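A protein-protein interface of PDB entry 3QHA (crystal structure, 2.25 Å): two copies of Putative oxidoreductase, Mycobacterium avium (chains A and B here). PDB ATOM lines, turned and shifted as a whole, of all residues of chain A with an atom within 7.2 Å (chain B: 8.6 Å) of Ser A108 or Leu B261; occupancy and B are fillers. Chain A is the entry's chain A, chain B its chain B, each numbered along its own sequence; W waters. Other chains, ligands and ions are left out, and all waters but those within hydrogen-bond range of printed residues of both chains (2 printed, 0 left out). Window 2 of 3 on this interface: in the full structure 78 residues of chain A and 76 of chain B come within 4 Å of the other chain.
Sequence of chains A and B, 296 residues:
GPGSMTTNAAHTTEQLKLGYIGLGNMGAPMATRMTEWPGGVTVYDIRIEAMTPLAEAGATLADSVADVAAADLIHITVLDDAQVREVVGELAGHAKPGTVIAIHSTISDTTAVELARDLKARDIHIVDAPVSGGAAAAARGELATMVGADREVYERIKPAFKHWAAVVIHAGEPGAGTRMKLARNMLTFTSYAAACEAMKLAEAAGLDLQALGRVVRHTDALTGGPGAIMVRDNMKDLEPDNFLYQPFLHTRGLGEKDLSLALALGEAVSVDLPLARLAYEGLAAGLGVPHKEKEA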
ATOM      1  N   ASP A  81     -10.139 -17.581 -27.250  1.00  0.00           N
ATOM      2  CA  ASP A  81     -10.115 -17.674 -25.786  1.00  0.00           C
ATOM      3  C   ASP A  81      -9.064 -16.746 -25.170  1.00  0.00           C
ATOM      4  O   ASP A  81      -9.358 -16.013 -24.223  1.00  0.00           O
ATOM      5  CB  ASP A  81      -9.855 -19.119 -25.337  1.00  0.00           C
ATOM      6  CG  ASP A  81     -10.873 -20.101 -25.899  1.00  0.00           C
ATOM      7  OD1 ASP A  81     -11.593 -20.742 -25.106  1.00  0.00           O
ATOM      8  OD2 ASP A  81     -10.958 -20.226 -27.141  1.00  0.00           O
ATOM      9  N   ARG A  85      -9.820 -13.871 -22.328  1.00  0.00           N
ATOM     10  CA  ARG A  85      -9.187 -13.830 -21.009  1.00  0.00           C
ATOM     11  C   ARG A  85      -8.528 -12.480 -20.776  1.00  0.00           C
ATOM     12  O   ARG A  85      -8.718 -11.862 -19.729  1.00  0.00           O
ATOM     13  CB  ARG A  85      -8.138 -14.933 -20.871  1.00  0.00           C
ATOM     14  CG  ARG A  85      -8.714 -16.328 -20.872  1.00  0.00           C
ATOM     15  CD  ARG A  85      -7.621 -17.377 -20.827  1.00  0.00           C
ATOM     16  NE  ARG A  85      -8.201 -18.714 -20.762  1.00  0.00           N
ATOM     17  CZ  ARG A  85      -8.721 -19.264 -19.665  1.00  0.00           C
ATOM     18  NH1 ARG A  85      -8.733 -18.609 -18.506  1.00  0.00           N
ATOM     19  NH2 ARG A  85      -9.231 -20.488 -19.725  1.00  0.00           N
ATOM     20  N   SER A 105     -18.348 -14.669 -28.676  1.00  0.00           N
ATOM     21  CA  SER A 105     -17.464 -15.235 -29.687  1.00  0.00           C
ATOM     22  C   SER A 105     -17.036 -16.643 -29.278  1.00  0.00           C
ATOM     23  O   SER A 105     -17.375 -17.113 -28.192  1.00  0.00           O
ATOM     24  CB  SER A 105     -16.256 -14.322 -29.900  1.00  0.00           C
ATOM     25  OG  SER A 105     -15.661 -13.954 -28.666  1.00  0.00           O
ATOM     26  N   THR A 106     -16.295 -17.313 -30.156  1.00  0.00           N
ATOM     27  CA  THR A 106     -15.970 -18.722 -29.977  1.00  0.00           C
ATOM     28  C   THR A 106     -14.970 -18.957 -28.844  1.00  0.00           C
ATOM     29  O   THR A 106     -13.884 -18.373 -28.826  1.00  0.00           O
ATOM     30  CB  THR A 106     -15.437 -19.340 -31.290  1.00  0.00           C
ATOM     31  OG1 THR A 106     -16.465 -19.281 -32.288  1.00  0.00           O
ATOM     32  CG2 THR A 106     -15.020 -20.794 -31.084  1.00  0.00           C
ATOM     33  N   ILE A 107     -15.371 -19.810 -27.902  1.00  0.00           N
ATOM     34  CA  ILE A 107     -14.539 -20.230 -26.775  1.00  0.00           C
ATOM     35  C   ILE A 107     -14.798 -21.699 -26.452  1.00  0.00           C
ATOM     36  O   ILE A 107     -15.843 -22.250 -26.809  1.00  0.00           O
ATOM     37  CB  ILE A 107     -14.837 -19.404 -25.500  1.00  0.00           C
ATOM     38  CG1 ILE A 107     -16.314 -19.519 -25.096  1.00  0.00           C
ATOM     39  CG2 ILE A 107     -14.454 -17.941 -25.702  1.00  0.00           C
ATOM     40  CD1 ILE A 107     -16.614 -18.946 -23.725  1.00  0.00           C
ATOM     41  N   SER A 108     -13.846 -22.330 -25.772  1.00  0.00           N
ATOM     42  CA  SER A 108     -14.075 -23.646 -25.188  1.00  0.00           C
ATOM     43  C   SER A 108     -14.983 -23.452 -23.978  1.00  0.00           C
ATOM     44  O   SER A 108     -14.907 -22.421 -23.306  1.00  0.00           O
ATOM     45  CB  SER A 108     -12.756 -24.296 -24.773  1.00  0.00           C
ATOM     46  OG  SER A 108     -11.965 -24.608 -25.909  1.00  0.00           O
ATOM     47  N   ASP A 109     -15.849 -24.424 -23.705  1.00  0.00           N
ATOM     48  CA  ASP A 109     -16.810 -24.284 -22.607  1.00  0.00           C
ATOM     49  C   ASP A 109     -16.100 -24.137 -21.254  1.00  0.00           C
ATOM     50  O   ASP A 109     -16.588 -23.440 -20.361  1.00  0.00           O
ATOM     51  CB  ASP A 109     -17.831 -25.436 -22.598  1.00  0.00           C
ATOM     52  CG  ASP A 109     -17.241 -26.761 -22.143  1.00  0.00           C
ATOM     53  OD1 ASP A 109     -17.937 -27.480 -21.396  1.00  0.00           O
ATOM     54  OD2 ASP A 109     -16.101 -27.093 -22.532  1.00  0.00           O
ATOM     55  N   THR A 110     -14.933 -24.766 -21.133  1.00  0.00           N
ATOM     56  CA  THR A 110     -14.119 -24.679 -19.926  1.00  0.00           C
ATOM     57  C   THR A 110     -13.612 -23.260 -19.635  1.00  0.00           C
ATOM     58  O   THR A 110     -13.401 -22.916 -18.474  1.00  0.00           O
ATOM     59  CB  THR A 110     -12.933 -25.664 -19.989  1.00  0.00           C
ATOM     60  OG1 THR A 110     -12.236 -25.501 -21.229  1.00  0.00           O
ATOM     61  CG2 THR A 110     -13.431 -27.098 -19.884  1.00  0.00           C
ATOM     62  N   THR A 111     -13.430 -22.440 -20.671  1.00  0.00           N
ATOM     63  CA  THR A 111     -13.045 -21.034 -20.487  1.00  0.00           C
ATOM     64  C   THR A 111     -14.135 -20.251 -19.750  1.00  0.00           C
ATOM     65  O   THR A 111     -13.837 -19.429 -18.879  1.00  0.00           O
ATOM     66  CB  THR A 111     -12.751 -20.334 -21.830  1.00  0.00           C
ATOM     67  OG1 THR A 111     -11.665 -20.996 -22.491  1.00  0.00           O
ATOM     68  CG2 THR A 111     -12.384 -18.865 -21.614  1.00  0.00           C
ATOM     69  N   ALA A 112     -15.391 -20.506 -20.108  1.00  0.00           N
ATOM     70  CA  ALA A 112     -16.528 -19.874 -19.446  1.00  0.00           C
ATOM     71  C   ALA A 112     -16.642 -20.339 -17.995  1.00  0.00           C
ATOM     72  O   ALA A 112     -16.843 -19.530 -17.092  1.00  0.00           O
ATOM     73  CB  ALA A 112     -17.818 -20.175 -20.200  1.00  0.00           C
ATOM     74  N   VAL A 113     -16.512 -21.644 -17.779  1.00  0.00           N
ATOM     75  CA  VAL A 113     -16.571 -22.206 -16.429  1.00  0.00           C
ATOM     76  C   VAL A 113     -15.487 -21.575 -15.556  1.00  0.00           C
ATOM     77  O   VAL A 113     -15.737 -21.179 -14.419  1.00  0.00           O
ATOM     78  CB  VAL A 113     -16.378 -23.740 -16.447  1.00  0.00           C
ATOM     79  CG1 VAL A 113     -16.265 -24.288 -15.029  1.00  0.00           C
ATOM     80  CG2 VAL A 113     -17.525 -24.412 -17.189  1.00  0.00           C
ATOM     81  N   ASP A 128     -21.577 -17.045 -20.747  1.00  0.00           N
ATOM     82  CA  ASP A 128     -21.289 -17.379 -22.145  1.00  0.00           C
ATOM     83  C   ASP A 128     -22.592 -17.395 -22.937  1.00  0.00           C
ATOM     84  O   ASP A 128     -23.531 -18.123 -22.602  1.00  0.00           O
ATOM     85  CB  ASP A 128     -20.485 -18.686 -22.313  1.00  0.00           C
ATOM     86  CG  ASP A 128     -21.193 -19.909 -21.764  1.00  0.00           C
ATOM     87  OD1 ASP A 128     -21.911 -19.785 -20.753  1.00  0.00           O
ATOM     88  OD2 ASP A 128     -20.997 -21.012 -22.324  1.00  0.00           O
ATOM     89  N   GLY A 175     -20.854 -22.193 -19.378  1.00  0.00           N
ATOM     90  CA  GLY A 175     -20.345 -23.329 -20.146  1.00  0.00           C
ATOM     91  C   GLY A 175     -21.433 -24.005 -20.970  1.00  0.00           C
ATOM     92  O   GLY A 175     -21.172 -24.479 -22.076  1.00  0.00           O
ATOM     93  N   THR A 178     -22.127 -22.436 -24.498  1.00  0.00           N
ATOM     94  CA  THR A 178     -21.126 -22.918 -25.445  1.00  0.00           C
ATOM     95  C   THR A 178     -21.419 -24.340 -25.912  1.00  0.00           C
ATOM     96  O   THR A 178     -21.339 -24.630 -27.106  1.00  0.00           O
ATOM     97  CB  THR A 178     -19.711 -22.869 -24.829  1.00  0.00           C
ATOM     98  OG1 THR A 178     -19.405 -21.522 -24.447  1.00  0.00           O
ATOM     99  CG2 THR A 178     -18.669 -23.366 -25.821  1.00  0.00           C
ATOM    100  N   ARG A 179     -21.766 -25.220 -24.978  1.00  0.00           N
ATOM    101  CA  ARG A 179     -22.051 -26.611 -25.320  1.00  0.00           C
ATOM    102  C   ARG A 179     -23.265 -26.729 -26.249  1.00  0.00           C
ATOM    103  O   ARG A 179     -23.250 -27.535 -27.181  1.00  0.00           O
ATOM    104  CB  ARG A 179     -22.231 -27.464 -24.058  1.00  0.00           C
ATOM    105  CG  ARG A 179     -20.928 -27.668 -23.275  1.00  0.00           C
ATOM    106  CD  ARG A 179     -21.053 -28.750 -22.210  1.00  0.00           C
ATOM    107  NE  ARG A 179     -21.868 -28.325 -21.072  1.00  0.00           N
ATOM    108  CZ  ARG A 179     -21.418 -27.678 -19.995  1.00  0.00           C
ATOM    109  NH1 ARG A 179     -20.133 -27.351 -19.863  1.00  0.00           N
ATOM    110  NH2 ARG A 179     -22.270 -27.348 -19.029  1.00  0.00           N
ATOM    111  N   LYS A 181     -24.278 -24.337 -28.309  1.00  0.00           N
ATOM    112  CA  LYS A 181     -23.769 -23.797 -29.569  1.00  0.00           C
ATOM    113  C   LYS A 181     -22.970 -24.845 -30.353  1.00  0.00           C
ATOM    114  O   LYS A 181     -23.053 -24.892 -31.581  1.00  0.00           O
ATOM    115  CB  LYS A 181     -22.892 -22.566 -29.319  1.00  0.00           C
ATOM    116  CG  LYS A 181     -22.476 -21.813 -30.590  1.00  0.00           C
ATOM    117  CD  LYS A 181     -21.053 -21.260 -30.502  1.00  0.00           C
ATOM    118  CE  LYS A 181     -20.020 -22.226 -31.072  1.00  0.00           C
ATOM    119  NZ  LYS A 181     -18.722 -21.539 -31.357  1.00  0.00           N
ATOM    120  N   LEU A 182     -22.197 -25.675 -29.655  1.00  0.00           N
ATOM    121  CA  LEU A 182     -21.367 -26.685 -30.325  1.00  0.00           C
ATOM    122  C   LEU A 182     -22.213 -27.789 -30.953  1.00  0.00           C
ATOM    123  O   LEU A 182     -21.887 -28.287 -32.028  1.00  0.00           O
ATOM    124  CB  LEU A 182     -20.334 -27.286 -29.368  1.00  0.00           C
ATOM    125  CG  LEU A 182     -19.227 -26.329 -28.914  1.00  0.00           C
ATOM    126  CD1 LEU A 182     -18.314 -27.011 -27.902  1.00  0.00           C
ATOM    127  CD2 LEU A 182     -18.424 -25.797 -30.095  1.00  0.00           C
ATOM    128  N   LEU B 201     -25.555 -35.724 -28.891  1.00  0.00           N
ATOM    129  CA  LEU B 201     -24.523 -34.944 -28.214  1.00  0.00           C
ATOM    130  C   LEU B 201     -25.120 -34.022 -27.154  1.00  0.00           C
ATOM    131  O   LEU B 201     -24.653 -33.990 -26.014  1.00  0.00           O
ATOM    132  CB  LEU B 201     -23.746 -34.100 -29.226  1.00  0.00           C
ATOM    133  CG  LEU B 201     -22.553 -33.315 -28.678  1.00  0.00           C
ATOM    134  CD1 LEU B 201     -21.525 -34.256 -28.063  1.00  0.00           C
ATOM    135  CD2 LEU B 201     -21.924 -32.473 -29.778  1.00  0.00           C
ATOM    136  N   LEU B 254     -14.277 -21.182 -39.335  1.00  0.00           N
ATOM    137  CA  LEU B 254     -15.339 -21.355 -38.340  1.00  0.00           C
ATOM    138  C   LEU B 254     -15.746 -22.820 -38.195  1.00  0.00           C
ATOM    139  O   LEU B 254     -15.898 -23.323 -37.078  1.00  0.00           O
ATOM    140  CB  LEU B 254     -16.584 -20.543 -38.717  1.00  0.00           C
ATOM    141  CG  LEU B 254     -16.520 -19.015 -38.670  1.00  0.00           C
ATOM    142  CD1 LEU B 254     -17.874 -18.445 -39.093  1.00  0.00           C
ATOM    143  CD2 LEU B 254     -16.132 -18.501 -37.285  1.00  0.00           C
ATOM    144  N   GLY B 255     -15.925 -23.491 -39.329  1.00  0.00           N
ATOM    145  CA  GLY B 255     -16.413 -24.870 -39.350  1.00  0.00           C
ATOM    146  C   GLY B 255     -15.461 -25.857 -38.708  1.00  0.00           C
ATOM    147  O   GLY B 255     -15.864 -26.666 -37.878  1.00  0.00           O
ATOM    148  N   GLU B 256     -14.194 -25.782 -39.095  1.00  0.00           N
ATOM    149  CA  GLU B 256     -13.167 -26.660 -38.547  1.00  0.00           C
ATOM    150  C   GLU B 256     -12.950 -26.416 -37.053  1.00  0.00           C
ATOM    151  O   GLU B 256     -12.698 -27.354 -36.297  1.00  0.00           O
ATOM    152  CB  GLU B 256     -11.863 -26.497 -39.331  1.00  0.00           C
ATOM    153  CG  GLU B 256     -11.963 -27.059 -40.748  1.00  0.00           C
ATOM    154  CD  GLU B 256     -10.673 -26.946 -41.536  1.00  0.00           C
ATOM    155  OE1 GLU B 256      -9.703 -26.354 -41.022  1.00  0.00           O
ATOM    156  OE2 GLU B 256     -10.630 -27.453 -42.677  1.00  0.00           O
ATOM    157  N   LYS B 257     -13.068 -25.163 -36.623  1.00  0.00           N
ATOM    158  CA  LYS B 257     -12.945 -24.842 -35.206  1.00  0.00           C
ATOM    159  C   LYS B 257     -14.138 -25.394 -34.412  1.00  0.00           C
ATOM    160  O   LYS B 257     -13.945 -26.063 -33.395  1.00  0.00           O
ATOM    161  CB  LYS B 257     -12.781 -23.331 -34.996  1.00  0.00           C
ATOM    162  CG  LYS B 257     -12.643 -22.893 -33.533  1.00  0.00           C
ATOM    163  CD  LYS B 257     -11.502 -23.605 -32.801  1.00  0.00           C
ATOM    164  CE  LYS B 257     -11.305 -23.038 -31.400  1.00  0.00           C
ATOM    165  NZ  LYS B 257     -10.470 -23.916 -30.528  1.00  0.00           N
ATOM    166  N   ASP B 258     -15.361 -25.136 -34.876  1.00  0.00           N
ATOM    167  CA  ASP B 258     -16.557 -25.639 -34.179  1.00  0.00           C
ATOM    168  C   ASP B 258     -16.648 -27.167 -34.208  1.00  0.00           C
ATOM    169  O   ASP B 258     -16.993 -27.785 -33.197  1.00  0.00           O
ATOM    170  CB  ASP B 258     -17.845 -25.019 -34.741  1.00  0.00           C
ATOM    171  CG  ASP B 258     -18.103 -23.610 -34.214  1.00  0.00           C
ATOM    172  OD1 ASP B 258     -17.396 -23.166 -33.284  1.00  0.00           O
ATOM    173  OD2 ASP B 258     -19.028 -22.944 -34.726  1.00  0.00           O
ATOM    174  N   LEU B 259     -16.333 -27.772 -35.351  1.00  0.00           N
ATOM    175  CA  LEU B 259     -16.358 -29.232 -35.470  1.00  0.00           C
ATOM    176  C   LEU B 259     -15.338 -29.892 -34.541  1.00  0.00           C
ATOM    177  O   LEU B 259     -15.654 -30.879 -33.879  1.00  0.00           O
ATOM    178  CB  LEU B 259     -16.139 -29.679 -36.922  1.00  0.00           C
ATOM    179  CG  LEU B 259     -17.353 -29.504 -37.842  1.00  0.00           C
ATOM    180  CD1 LEU B 259     -16.989 -29.786 -39.296  1.00  0.00           C
ATOM    181  CD2 LEU B 259     -18.507 -30.395 -37.400  1.00  0.00           C
ATOM    182  N   SER B 260     -14.130 -29.337 -34.475  1.00  0.00           N
ATOM    183  CA  SER B 260     -13.097 -29.869 -33.588  1.00  0.00           C
ATOM    184  C   SER B 260     -13.520 -29.762 -32.124  1.00  0.00           C
ATOM    185  O   SER B 260     -13.347 -30.711 -31.355  1.00  0.00           O
ATOM    186  CB  SER B 260     -11.763 -29.151 -33.803  1.00  0.00           C
ATOM    187  OG  SER B 260     -11.870 -27.774 -33.490  1.00  0.00           O
ATOM    188  N   LEU B 261     -14.076 -28.612 -31.748  1.00  0.00           N
ATOM    189  CA  LEU B 261     -14.609 -28.424 -30.398  1.00  0.00           C
ATOM    190  C   LEU B 261     -15.755 -29.393 -30.121  1.00  0.00           C
ATOM    191  O   LEU B 261     -15.839 -29.966 -29.034  1.00  0.00           O
ATOM    192  CB  LEU B 261     -15.084 -26.983 -30.185  1.00  0.00           C
ATOM    193  CG  LEU B 261     -13.991 -25.926 -29.981  1.00  0.00           C
ATOM    194  CD1 LEU B 261     -14.590 -24.530 -30.005  1.00  0.00           C
ATOM    195  CD2 LEU B 261     -13.236 -26.160 -28.680  1.00  0.00           C
ATOM    196  N   ALA B 262     -16.628 -29.578 -31.107  1.00  0.00           N
ATOM    197  CA  ALA B 262     -17.749 -30.505 -30.970  1.00  0.00           C
ATOM    198  C   ALA B 262     -17.253 -31.941 -30.798  1.00  0.00           C
ATOM    199  O   ALA B 262     -17.800 -32.695 -29.997  1.00  0.00           O
ATOM    200  CB  ALA B 262     -18.679 -30.404 -32.168  1.00  0.00           C
ATOM    201  N   LEU B 263     -16.211 -32.308 -31.541  1.00  0.00           N
ATOM    202  CA  LEU B 263     -15.636 -33.653 -31.447  1.00  0.00           C
ATOM    203  C   LEU B 263     -14.969 -33.894 -30.091  1.00  0.00           C
ATOM    204  O   LEU B 263     -15.013 -35.005 -29.561  1.00  0.00           O
ATOM    205  CB  LEU B 263     -14.632 -33.891 -32.576  1.00  0.00           C
ATOM    206  CG  LEU B 263     -15.254 -34.085 -33.961  1.00  0.00           C
ATOM    207  CD1 LEU B 263     -14.216 -33.862 -35.055  1.00  0.00           C
ATOM    208  CD2 LEU B 263     -15.883 -35.470 -34.087  1.00  0.00           C
ATOM    209  N   ALA B 264     -14.355 -32.850 -29.539  1.00  0.00           N
ATOM    210  CA  ALA B 264     -13.722 -32.936 -28.227  1.00  0.00           C
ATOM    211  C   ALA B 264     -14.776 -33.067 -27.134  1.00  0.00           C
ATOM    212  O   ALA B 264     -14.607 -33.857 -26.199  1.00  0.00           O
ATOM    213  CB  ALA B 264     -12.842 -31.718 -27.975  1.00  0.00           C
ATOM    214  N   LEU B 265     -15.860 -32.299 -27.254  1.00  0.00           N
ATOM    215  CA  LEU B 265     -16.985 -32.416 -26.324  1.00  0.00           C
ATOM    216  C   LEU B 265     -17.560 -33.832 -26.362  1.00  0.00           C
ATOM    217  O   LEU B 265     -17.921 -34.386 -25.324  1.00  0.00           O
ATOM    218  CB  LEU B 265     -18.083 -31.391 -26.642  1.00  0.00           C
ATOM    219  CG  LEU B 265     -19.341 -31.427 -25.758  1.00  0.00           C
ATOM    220  CD1 LEU B 265     -19.009 -31.112 -24.303  1.00  0.00           C
ATOM    221  CD2 LEU B 265     -20.397 -30.465 -26.288  1.00  0.00           C
ATOM    222  N   GLY B 266     -17.635 -34.410 -27.560  1.00  0.00           N
ATOM    223  CA  GLY B 266     -18.151 -35.767 -27.737  1.00  0.00           C
ATOM    224  C   GLY B 266     -17.282 -36.819 -27.073  1.00  0.00           C
ATOM    225  O   GLY B 266     -17.790 -37.805 -26.542  1.00  0.00           O
ATOM    226  N   GLU B 267     -15.969 -36.611 -27.108  1.00  0.00           N
ATOM    227  CA  GLU B 267     -15.036 -37.468 -26.384  1.00  0.00           C
ATOM    228  C   GLU B 267     -15.255 -37.334 -24.876  1.00  0.00           C
ATOM    229  O   GLU B 267     -15.177 -38.321 -24.141  1.00  0.00           O
ATOM    230  CB  GLU B 267     -13.589 -37.112 -26.743  1.00  0.00           C
ATOM    231  N   ALA B 268     -15.541 -36.112 -24.430  1.00  0.00           N
ATOM    232  CA  ALA B 268     -15.744 -35.822 -23.009  1.00  0.00           C
ATOM    233  C   ALA B 268     -17.026 -36.433 -22.442  1.00  0.00           C
ATOM    234  O   ALA B 268     -17.045 -36.852 -21.286  1.00  0.00           O
ATOM    235  CB  ALA B 268     -15.733 -34.315 -22.770  1.00  0.00           C
ATOM    236  N   LEU B 273     -19.375 -39.532 -32.699  1.00  0.00           N
ATOM    237  CA  LEU B 273     -19.875 -38.529 -33.646  1.00  0.00           C
ATOM    238  C   LEU B 273     -19.293 -38.759 -35.047  1.00  0.00           C
ATOM    239  O   LEU B 273     -18.558 -37.914 -35.566  1.00  0.00           O
ATOM    240  CB  LEU B 273     -19.513 -37.125 -33.152  1.00  0.00           C
ATOM    241  CG  LEU B 273     -20.046 -36.720 -31.778  1.00  0.00           C
ATOM    242  CD1 LEU B 273     -19.441 -35.387 -31.347  1.00  0.00           C
ATOM    243  CD2 LEU B 273     -21.567 -36.651 -31.788  1.00  0.00           C
ATOM    244  N   TYR B 280     -15.697 -32.971 -40.629  1.00  0.00           N
ATOM    245  CA  TYR B 280     -14.468 -32.280 -40.245  1.00  0.00           C
ATOM    246  C   TYR B 280     -13.316 -32.522 -41.228  1.00  0.00           C
ATOM    247  O   TYR B 280     -12.615 -31.582 -41.602  1.00  0.00           O
ATOM    248  CB  TYR B 280     -14.057 -32.705 -38.831  1.00  0.00           C
ATOM    249  CG  TYR B 280     -12.769 -32.086 -38.338  1.00  0.00           C
ATOM    250  CD1 TYR B 280     -12.712 -30.741 -37.984  1.00  0.00           C
ATOM    251  CD2 TYR B 280     -11.610 -32.847 -38.215  1.00  0.00           C
ATOM    252  CE1 TYR B 280     -11.536 -30.169 -37.528  1.00  0.00           C
ATOM    253  CE2 TYR B 280     -10.425 -32.279 -37.758  1.00  0.00           C
ATOM    254  CZ  TYR B 280     -10.398 -30.939 -37.416  1.00  0.00           C
ATOM    255  OH  TYR B 280      -9.233 -30.366 -36.961  1.00  0.00           O
HETATM  256  O   HOH W   1     -15.939 -20.887 -34.461  1.00  0.00           O
HETATM  257  O   HOH W   2     -11.230 -22.954 -27.905  1.00  0.00           O
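Of the 18 printed residues of chain B, 4 touch a printed residue of chain A.
Hydrophobic or aromatic side chains of chain B that line the printed part of chain A: Leu B261, Ala B262 and Leu B265.
Hydrophobic or aromatic side chains of chain A within 4 Å of the printed part of chain B: Leu A182.
Among the printed residues, 7 pairs touch across the chains.
Among the printed residues, Asp or Glu carboxylates within 4 Å of a Lys or Arg side-chain nitrogen of the other chain: Lys A181 with Asp B258.
No position is printed for both chains.
Of the 7 pairs that touch across the chains among the printed residues, none has its exchanged pair printed and touching as well.
Ser A108 touches just one residue of chain B: Leu B261 (3.4 Å).
Leu B261 touches just these residues of chain A: Thr A106, Ser A108 and Leu A182.
No residue of chain B comes within 4 Å of Ile A107.
Printed residues of chain A within 4 Å of Leu B265: Arg A179.
Printed residues of chain A within 4 Å of Asp B258: Lys A181 (2.8 Å) and Leu A182 (3.95 Å).
Printed residues of chain B within 4 Å of Thr A106: Leu B261.
Of the printed residues of chain B, Arg A179 touches Leu B265 (3.8 Å).
The nearest residue of chain A that does not touch Leu B261 is Ile A107 (4.1 Å).
NZ of Lys A181 lies within salt-bridge range of OD1 of Asp B258 (2.8 Å).
Water W2 lies within hydrogen-bond range of the side-chain hydroxyl of Ser A108, the side-chain carboxylate of Asp A81 and the side-chain amino group of Lys B257.
Water W1 lies within hydrogen-bond range of the side-chain hydroxyl (OG1) of Thr A106 (2.8 Å) and the side-chain carboxylate (OD1) of Asp B258 (2.9 Å).
Leu B261 touches Thr A106 (CD1 to CG2, 3.9 Å).
Ser A108 touches Leu B261 (OG to CD2, 3.4 Å).
Leu B265 touches Arg A179.
Leu A182 touches Asp B258.
Leu A182 touches Leu B261 (CD2 to CB, 3.5 Å).
Ala B262 touches Leu A182.
OD1 of Asp A81 lies within hydrogen-bond range of N of Ser A108 (2.8 Å).
The side-chain hydroxyl of Thr A106 lies within hydrogen-bond range of the side-chain amino group of Lys A181.
The guanidinium group (NH1) of Arg A179 is in salt-bridge range of the side-chain carboxylate (OD1) of Asp A109, at 2.7 Å.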
